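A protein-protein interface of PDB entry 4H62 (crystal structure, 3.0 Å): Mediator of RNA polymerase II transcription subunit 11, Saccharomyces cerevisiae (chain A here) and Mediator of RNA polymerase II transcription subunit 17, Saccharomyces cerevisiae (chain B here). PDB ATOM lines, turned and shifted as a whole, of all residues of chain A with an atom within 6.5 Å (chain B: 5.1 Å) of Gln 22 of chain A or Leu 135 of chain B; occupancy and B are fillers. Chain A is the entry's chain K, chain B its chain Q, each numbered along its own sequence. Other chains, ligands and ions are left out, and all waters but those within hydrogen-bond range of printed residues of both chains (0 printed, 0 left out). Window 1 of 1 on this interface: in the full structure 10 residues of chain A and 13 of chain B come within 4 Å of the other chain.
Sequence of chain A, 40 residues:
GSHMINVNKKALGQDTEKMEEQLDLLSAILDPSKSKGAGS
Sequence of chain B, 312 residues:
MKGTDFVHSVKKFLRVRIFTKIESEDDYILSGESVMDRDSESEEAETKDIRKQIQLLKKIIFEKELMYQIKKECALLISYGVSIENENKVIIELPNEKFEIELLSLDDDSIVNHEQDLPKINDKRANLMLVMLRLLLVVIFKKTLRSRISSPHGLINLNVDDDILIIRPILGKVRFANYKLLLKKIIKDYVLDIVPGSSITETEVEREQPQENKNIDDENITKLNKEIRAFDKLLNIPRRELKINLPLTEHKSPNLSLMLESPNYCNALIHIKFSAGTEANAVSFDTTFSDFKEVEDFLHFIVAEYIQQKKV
Among the printed residues, merely in contact across the chains: Lys 18 of chain A with Val 138 of chain B (3.9 Å), Met 19 of chain A with Val 138 of chain B (3.8 Å), Met 19 of chain A with Phe 231 of chain B (3.9 Å), Gln 22 of chain A with Val 131 of chain B (3.5 Å), Gln 22 of chain A with Leu 135 of chain B (3.8 Å), Leu 25 of chain A with Val 131 of chain B (3.9 Å), Leu 25 of chain A with Arg 134 of chain B (3.7 Å), Leu 26 of chain A with Val 131 of chain B (3.6 Å) and Leu 26 of chain A with Leu 135 of chain B (3.6 Å).
Hydrophobic or aromatic side chains of chain B within 4 Å of the printed part of chain A: Val 131, Leu 135, Val 138 and Phe 231. Of the 11 printed residues of chain A, 5 touch a printed residue of chain B. Hydrophobic or aromatic side chains of chain A that line the printed part of chain B: Met 19, Leu 25 and Leu 26. Along chain A the printed residues that touch a printed residue of chain B span positions 18 to 26. Among the printed residues, 10 pairs touch across the chains. Among the printed residues, no Asp or Glu carboxylate lies within 4 Å of a Lys or Arg side-chain nitrogen of the other chain.
Of the printed residues of chain B, Lys 18 of chain A touches Val 138. Of the printed residues of chain B, Met 19 of chain A touches Val 138 and Phe 231. Glu 20 of chain A touches none of the printed residues of chain B. Of chain B, only Val 131 (3.5 Å), Arg 134 (3.1 Å) and Leu 135 (3.8 Å) come within 4 Å of Gln 22 of chain A. Of the printed residues of chain B, Leu 25 of chain A touches Val 131 and Arg 134. Leu 135 of chain B touches just these residues of chain A: Gln 22 (3.8 Å) and Leu 26 (3.6 Å). Leu 136 of chain B touches none of the printed residues of chain A. Printed residues of chain A within 4 Å of Val 138 of chain B: Lys 18 and Met 19. Of the printed residues of chain A, Phe 231 of chain B touches Met 19 (3.9 Å).
NZ of Lys 18 of chain A lies within salt-bridge range of OE2 of Glu 21 of chain A (2.9 Å). The side-chain carboxylate (OE2) of Glu 21 of chain A sits at hydrogen-bond distance from the side-chain amide nitrogen (NE2) of Gln 22 of chain A (3.2 Å).
OE1 of Gln 22 of chain A is in hydrogen-bond range of NH1 of Arg 134 of chain B (3.1 Å).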
ATOM      1  N   GLU A  17      -5.016  28.393  -3.916  1.00  0.00           N
ATOM      2  CA  GLU A  17      -5.128  27.289  -4.868  1.00  0.00           C
ATOM      3  C   GLU A  17      -3.776  26.591  -5.054  1.00  0.00           C
ATOM      4  O   GLU A  17      -3.710  25.363  -5.137  1.00  0.00           O
ATOM      5  CB  GLU A  17      -5.715  27.776  -6.200  1.00  0.00           C
ATOM      6  CG  GLU A  17      -4.786  27.681  -7.406  1.00  0.00           C
ATOM      7  CD  GLU A  17      -5.177  28.636  -8.528  1.00  0.00           C
ATOM      8  OE1 GLU A  17      -6.206  28.386  -9.201  1.00  0.00           O
ATOM      9  OE2 GLU A  17      -4.452  29.637  -8.730  1.00  0.00           O
ATOM     10  N   LYS A  18      -2.703  27.378  -5.092  1.00  0.00           N
ATOM     11  CA  LYS A  18      -1.355  26.834  -5.216  1.00  0.00           C
ATOM     12  C   LYS A  18      -1.052  25.949  -4.015  1.00  0.00           C
ATOM     13  O   LYS A  18      -0.614  24.807  -4.167  1.00  0.00           O
ATOM     14  CB  LYS A  18      -0.325  27.968  -5.324  1.00  0.00           C
ATOM     15  CG  LYS A  18       1.102  27.512  -5.617  1.00  0.00           C
ATOM     16  CD  LYS A  18       1.171  26.652  -6.872  1.00  0.00           C
ATOM     17  CE  LYS A  18       2.574  26.104  -7.110  1.00  0.00           C
ATOM     18  NZ  LYS A  18       2.591  25.017  -8.139  1.00  0.00           N
ATOM     19  N   MET A  19      -1.312  26.483  -2.825  1.00  0.00           N
ATOM     20  CA  MET A  19      -1.077  25.778  -1.567  1.00  0.00           C
ATOM     21  C   MET A  19      -1.773  24.421  -1.481  1.00  0.00           C
ATOM     22  O   MET A  19      -1.188  23.453  -1.004  1.00  0.00           O
ATOM     23  CB  MET A  19      -1.523  26.644  -0.394  1.00  0.00           C
ATOM     24  CG  MET A  19      -1.213  26.052   0.969  1.00  0.00           C
ATOM     25  SD  MET A  19      -2.096  27.043   2.393  1.00  0.00           S
ATOM     26  CE  MET A  19      -3.938  26.513   2.021  1.00  0.00           C
ATOM     27  N   GLU A  20      -3.021  24.354  -1.934  1.00  0.00           N
ATOM     28  CA  GLU A  20      -3.773  23.111  -1.871  1.00  0.00           C
ATOM     29  C   GLU A  20      -3.158  22.087  -2.817  1.00  0.00           C
ATOM     30  O   GLU A  20      -3.197  20.884  -2.558  1.00  0.00           O
ATOM     31  CB  GLU A  20      -5.241  23.340  -2.236  1.00  0.00           C
ATOM     32  CG  GLU A  20      -5.958  24.412  -1.419  1.00  0.00           C
ATOM     33  CD  GLU A  20      -6.475  23.913  -0.087  1.00  0.00           C
ATOM     34  OE1 GLU A  20      -6.521  22.678   0.109  1.00  0.00           O
ATOM     35  OE2 GLU A  20      -6.838  24.760   0.760  1.00  0.00           O
ATOM     36  N   GLU A  21      -2.590  22.577  -3.915  1.00  0.00           N
ATOM     37  CA  GLU A  21      -1.911  21.723  -4.886  1.00  0.00           C
ATOM     38  C   GLU A  21      -0.707  21.040  -4.232  1.00  0.00           C
ATOM     39  O   GLU A  21      -0.540  19.823  -4.327  1.00  0.00           O
ATOM     40  CB  GLU A  21      -1.484  22.556  -6.106  1.00  0.00           C
ATOM     41  CG  GLU A  21      -0.570  21.860  -7.114  1.00  0.00           C
ATOM     42  CD  GLU A  21       0.010  22.834  -8.134  1.00  0.00           C
ATOM     43  OE1 GLU A  21      -0.642  23.861  -8.411  1.00  0.00           O
ATOM     44  OE2 GLU A  21       1.120  22.585  -8.653  1.00  0.00           O
ATOM     45  N   GLN A  22       0.109  21.831  -3.543  1.00  0.00           N
ATOM     46  CA  GLN A  22       1.324  21.327  -2.916  1.00  0.00           C
ATOM     47  C   GLN A  22       1.053  20.402  -1.732  1.00  0.00           C
ATOM     48  O   GLN A  22       1.716  19.380  -1.571  1.00  0.00           O
ATOM     49  CB  GLN A  22       2.214  22.494  -2.497  1.00  0.00           C
ATOM     50  CG  GLN A  22       2.735  23.281  -3.679  1.00  0.00           C
ATOM     51  CD  GLN A  22       3.348  22.376  -4.734  1.00  0.00           C
ATOM     52  OE1 GLN A  22       4.410  21.791  -4.521  1.00  0.00           O
ATOM     53  NE2 GLN A  22       2.673  22.243  -5.869  1.00  0.00           N
ATOM     54  N   LEU A  23       0.081  20.763  -0.904  1.00  0.00           N
ATOM     55  CA  LEU A  23      -0.311  19.915   0.216  1.00  0.00           C
ATOM     56  C   LEU A  23      -0.803  18.562  -0.302  1.00  0.00           C
ATOM     57  O   LEU A  23      -0.406  17.509   0.203  1.00  0.00           O
ATOM     58  CB  LEU A  23      -1.392  20.602   1.054  1.00  0.00           C
ATOM     59  CG  LEU A  23      -0.949  21.871   1.786  1.00  0.00           C
ATOM     60  CD1 LEU A  23      -2.128  22.648   2.325  1.00  0.00           C
ATOM     61  CD2 LEU A  23       0.000  21.512   2.913  1.00  0.00           C
ATOM     62  N   ASP A  24      -1.670  18.606  -1.312  1.00  0.00           N
ATOM     63  CA  ASP A  24      -2.115  17.403  -2.000  1.00  0.00           C
ATOM     64  C   ASP A  24      -0.902  16.598  -2.436  1.00  0.00           C
ATOM     65  O   ASP A  24      -0.813  15.396  -2.188  1.00  0.00           O
ATOM     66  CB  ASP A  24      -2.956  17.768  -3.226  1.00  0.00           C
ATOM     67  CG  ASP A  24      -4.447  17.716  -2.951  1.00  0.00           C
ATOM     68  OD1 ASP A  24      -4.869  16.876  -2.127  1.00  0.00           O
ATOM     69  OD2 ASP A  24      -5.198  18.508  -3.567  1.00  0.00           O
ATOM     70  N   LEU A  25       0.036  17.287  -3.076  1.00  0.00           N
ATOM     71  CA  LEU A  25       1.267  16.682  -3.558  1.00  0.00           C
ATOM     72  C   LEU A  25       2.050  16.068  -2.396  1.00  0.00           C
ATOM     73  O   LEU A  25       2.596  14.970  -2.507  1.00  0.00           O
ATOM     74  CB  LEU A  25       2.114  17.747  -4.265  1.00  0.00           C
ATOM     75  CG  LEU A  25       2.958  17.418  -5.500  1.00  0.00           C
ATOM     76  CD1 LEU A  25       3.838  18.614  -5.839  1.00  0.00           C
ATOM     77  CD2 LEU A  25       3.802  16.167  -5.301  1.00  0.00           C
ATOM     78  N   LEU A  26       2.089  16.780  -1.276  1.00  0.00           N
ATOM     79  CA  LEU A  26       2.893  16.350  -0.140  1.00  0.00           C
ATOM     80  C   LEU A  26       2.318  15.115   0.551  1.00  0.00           C
ATOM     81  O   LEU A  26       3.053  14.182   0.867  1.00  0.00           O
ATOM     82  CB  LEU A  26       3.054  17.494   0.860  1.00  0.00           C
ATOM     83  CG  LEU A  26       4.382  17.525   1.613  1.00  0.00           C
ATOM     84  CD1 LEU A  26       4.632  18.905   2.168  1.00  0.00           C
ATOM     85  CD2 LEU A  26       4.410  16.502   2.733  1.00  0.00           C
ATOM     86  N   SER A  27       1.012  15.110   0.795  1.00  0.00           N
ATOM     87  CA  SER A  27       0.375  13.985   1.469  1.00  0.00           C
ATOM     88  C   SER A  27       0.441  12.761   0.578  1.00  0.00           C
ATOM     89  O   SER A  27       0.445  11.627   1.059  1.00  0.00           O
ATOM     90  CB  SER A  27      -1.083  14.297   1.799  1.00  0.00           C
ATOM     91  OG  SER A  27      -1.869  14.324   0.623  1.00  0.00           O
ATOM     92  N   VAL B 131       8.713  20.127  -2.489  1.00  0.00           N
ATOM     93  CA  VAL B 131       7.374  20.596  -2.141  1.00  0.00           C
ATOM     94  C   VAL B 131       7.431  21.644  -1.038  1.00  0.00           C
ATOM     95  O   VAL B 131       6.753  22.673  -1.106  1.00  0.00           O
ATOM     96  CB  VAL B 131       6.474  19.443  -1.684  1.00  0.00           C
ATOM     97  CG1 VAL B 131       5.149  19.976  -1.181  1.00  0.00           C
ATOM     98  CG2 VAL B 131       6.259  18.458  -2.823  1.00  0.00           C
ATOM     99  N   MET B 132       8.242  21.377  -0.020  1.00  0.00           N
ATOM    100  CA  MET B 132       8.460  22.344   1.043  1.00  0.00           C
ATOM    101  C   MET B 132       8.941  23.678   0.483  1.00  0.00           C
ATOM    102  O   MET B 132       8.463  24.721   0.905  1.00  0.00           O
ATOM    103  CB  MET B 132       9.443  21.806   2.076  1.00  0.00           C
ATOM    104  CG  MET B 132       8.796  20.985   3.193  1.00  0.00           C
ATOM    105  SD  MET B 132      10.083  20.369   4.549  1.00  0.00           S
ATOM    106  CE  MET B 132      11.051  19.118   3.446  1.00  0.00           C
ATOM    107  N   LEU B 133       9.861  23.652  -0.478  1.00  0.00           N
ATOM    108  CA  LEU B 133      10.375  24.895  -1.051  1.00  0.00           C
ATOM    109  C   LEU B 133       9.241  25.748  -1.591  1.00  0.00           C
ATOM    110  O   LEU B 133       9.077  26.889  -1.164  1.00  0.00           O
ATOM    111  CB  LEU B 133      11.382  24.630  -2.168  1.00  0.00           C
ATOM    112  CG  LEU B 133      12.802  24.136  -1.878  1.00  0.00           C
ATOM    113  CD1 LEU B 133      13.524  23.916  -3.198  1.00  0.00           C
ATOM    114  CD2 LEU B 133      13.600  25.082  -0.985  1.00  0.00           C
ATOM    115  N   ARG B 134       8.456  25.183  -2.511  1.00  0.00           N
ATOM    116  CA  ARG B 134       7.280  25.853  -3.083  1.00  0.00           C
ATOM    117  C   ARG B 134       6.313  26.390  -2.019  1.00  0.00           C
ATOM    118  O   ARG B 134       5.841  27.536  -2.094  1.00  0.00           O
ATOM    119  CB  ARG B 134       6.508  24.897  -3.992  1.00  0.00           C
ATOM    120  CG  ARG B 134       7.319  24.292  -5.114  1.00  0.00           C
ATOM    121  CD  ARG B 134       6.404  23.662  -6.155  1.00  0.00           C
ATOM    122  NE  ARG B 134       7.153  22.981  -7.203  1.00  0.00           N
ATOM    123  CZ  ARG B 134       7.269  21.661  -7.297  1.00  0.00           C
ATOM    124  NH1 ARG B 134       6.669  20.881  -6.406  1.00  0.00           N
ATOM    125  NH2 ARG B 134       7.977  21.119  -8.286  1.00  0.00           N
ATOM    126  N   LEU B 135       6.015  25.546  -1.038  1.00  0.00           N
ATOM    127  CA  LEU B 135       5.148  25.919   0.064  1.00  0.00           C
ATOM    128  C   LEU B 135       5.682  27.144   0.800  1.00  0.00           C
ATOM    129  O   LEU B 135       4.912  27.997   1.250  1.00  0.00           O
ATOM    130  CB  LEU B 135       5.006  24.749   1.032  1.00  0.00           C
ATOM    131  CG  LEU B 135       3.977  23.703   0.628  1.00  0.00           C
ATOM    132  CD1 LEU B 135       4.234  22.419   1.366  1.00  0.00           C
ATOM    133  CD2 LEU B 135       2.584  24.218   0.941  1.00  0.00           C
ATOM    134  N   LEU B 136       6.997  27.242   0.920  1.00  0.00           N
ATOM    135  CA  LEU B 136       7.561  28.375   1.632  1.00  0.00           C
ATOM    136  C   LEU B 136       7.313  29.678   0.877  1.00  0.00           C
ATOM    137  O   LEU B 136       7.010  30.706   1.495  1.00  0.00           O
ATOM    138  CB  LEU B 136       9.040  28.152   1.949  1.00  0.00           C
ATOM    139  CG  LEU B 136       9.159  27.190   3.138  1.00  0.00           C
ATOM    140  CD1 LEU B 136      10.592  26.967   3.558  1.00  0.00           C
ATOM    141  CD2 LEU B 136       8.337  27.699   4.304  1.00  0.00           C
ATOM    142  N   LEU B 137       7.403  29.615  -0.453  1.00  0.00           N
ATOM    143  CA  LEU B 137       7.107  30.767  -1.295  1.00  0.00           C
ATOM    144  C   LEU B 137       5.639  31.196  -1.172  1.00  0.00           C
ATOM    145  O   LEU B 137       5.323  32.395  -1.119  1.00  0.00           O
ATOM    146  CB  LEU B 137       7.450  30.484  -2.759  1.00  0.00           C
ATOM    147  CG  LEU B 137       7.493  31.729  -3.658  1.00  0.00           C
ATOM    148  CD1 LEU B 137       8.478  32.777  -3.130  1.00  0.00           C
ATOM    149  CD2 LEU B 137       7.813  31.378  -5.121  1.00  0.00           C
ATOM    150  N   VAL B 138       4.748  30.209  -1.133  1.00  0.00           N
ATOM    151  CA  VAL B 138       3.322  30.469  -0.974  1.00  0.00           C
ATOM    152  C   VAL B 138       3.065  31.252   0.302  1.00  0.00           C
ATOM    153  O   VAL B 138       2.331  32.233   0.288  1.00  0.00           O
ATOM    154  CB  VAL B 138       2.504  29.169  -0.928  1.00  0.00           C
ATOM    155  CG1 VAL B 138       1.032  29.475  -0.757  1.00  0.00           C
ATOM    156  CG2 VAL B 138       2.732  28.357  -2.183  1.00  0.00           C
ATOM    157  N   VAL B 139       3.683  30.821   1.401  1.00  0.00           N
ATOM    158  CA  VAL B 139       3.537  31.532   2.666  1.00  0.00           C
ATOM    159  C   VAL B 139       4.054  32.968   2.533  1.00  0.00           C
ATOM    160  O   VAL B 139       3.459  33.912   3.060  1.00  0.00           O
ATOM    161  CB  VAL B 139       4.247  30.813   3.831  1.00  0.00           C
ATOM    162  CG1 VAL B 139       4.124  31.622   5.114  1.00  0.00           C
ATOM    163  CG2 VAL B 139       3.656  29.434   4.037  1.00  0.00           C
ATOM    164  N   PHE B 231       1.734  26.751   9.168  1.00  0.00           N
ATOM    165  CA  PHE B 231       3.143  26.528   8.821  1.00  0.00           C
ATOM    166  C   PHE B 231       4.114  27.032   9.884  1.00  0.00           C
ATOM    167  O   PHE B 231       5.319  27.045   9.665  1.00  0.00           O
ATOM    168  CB  PHE B 231       3.490  27.138   7.458  1.00  0.00           C
ATOM    169  CG  PHE B 231       2.679  26.590   6.330  1.00  0.00           C
ATOM    170  CD1 PHE B 231       1.402  27.069   6.086  1.00  0.00           C
ATOM    171  CD2 PHE B 231       3.182  25.597   5.521  1.00  0.00           C
ATOM    172  CE1 PHE B 231       0.643  26.565   5.057  1.00  0.00           C
ATOM    173  CE2 PHE B 231       2.432  25.087   4.486  1.00  0.00           C
ATOM    174  CZ  PHE B 231       1.160  25.573   4.252  1.00  0.00           C
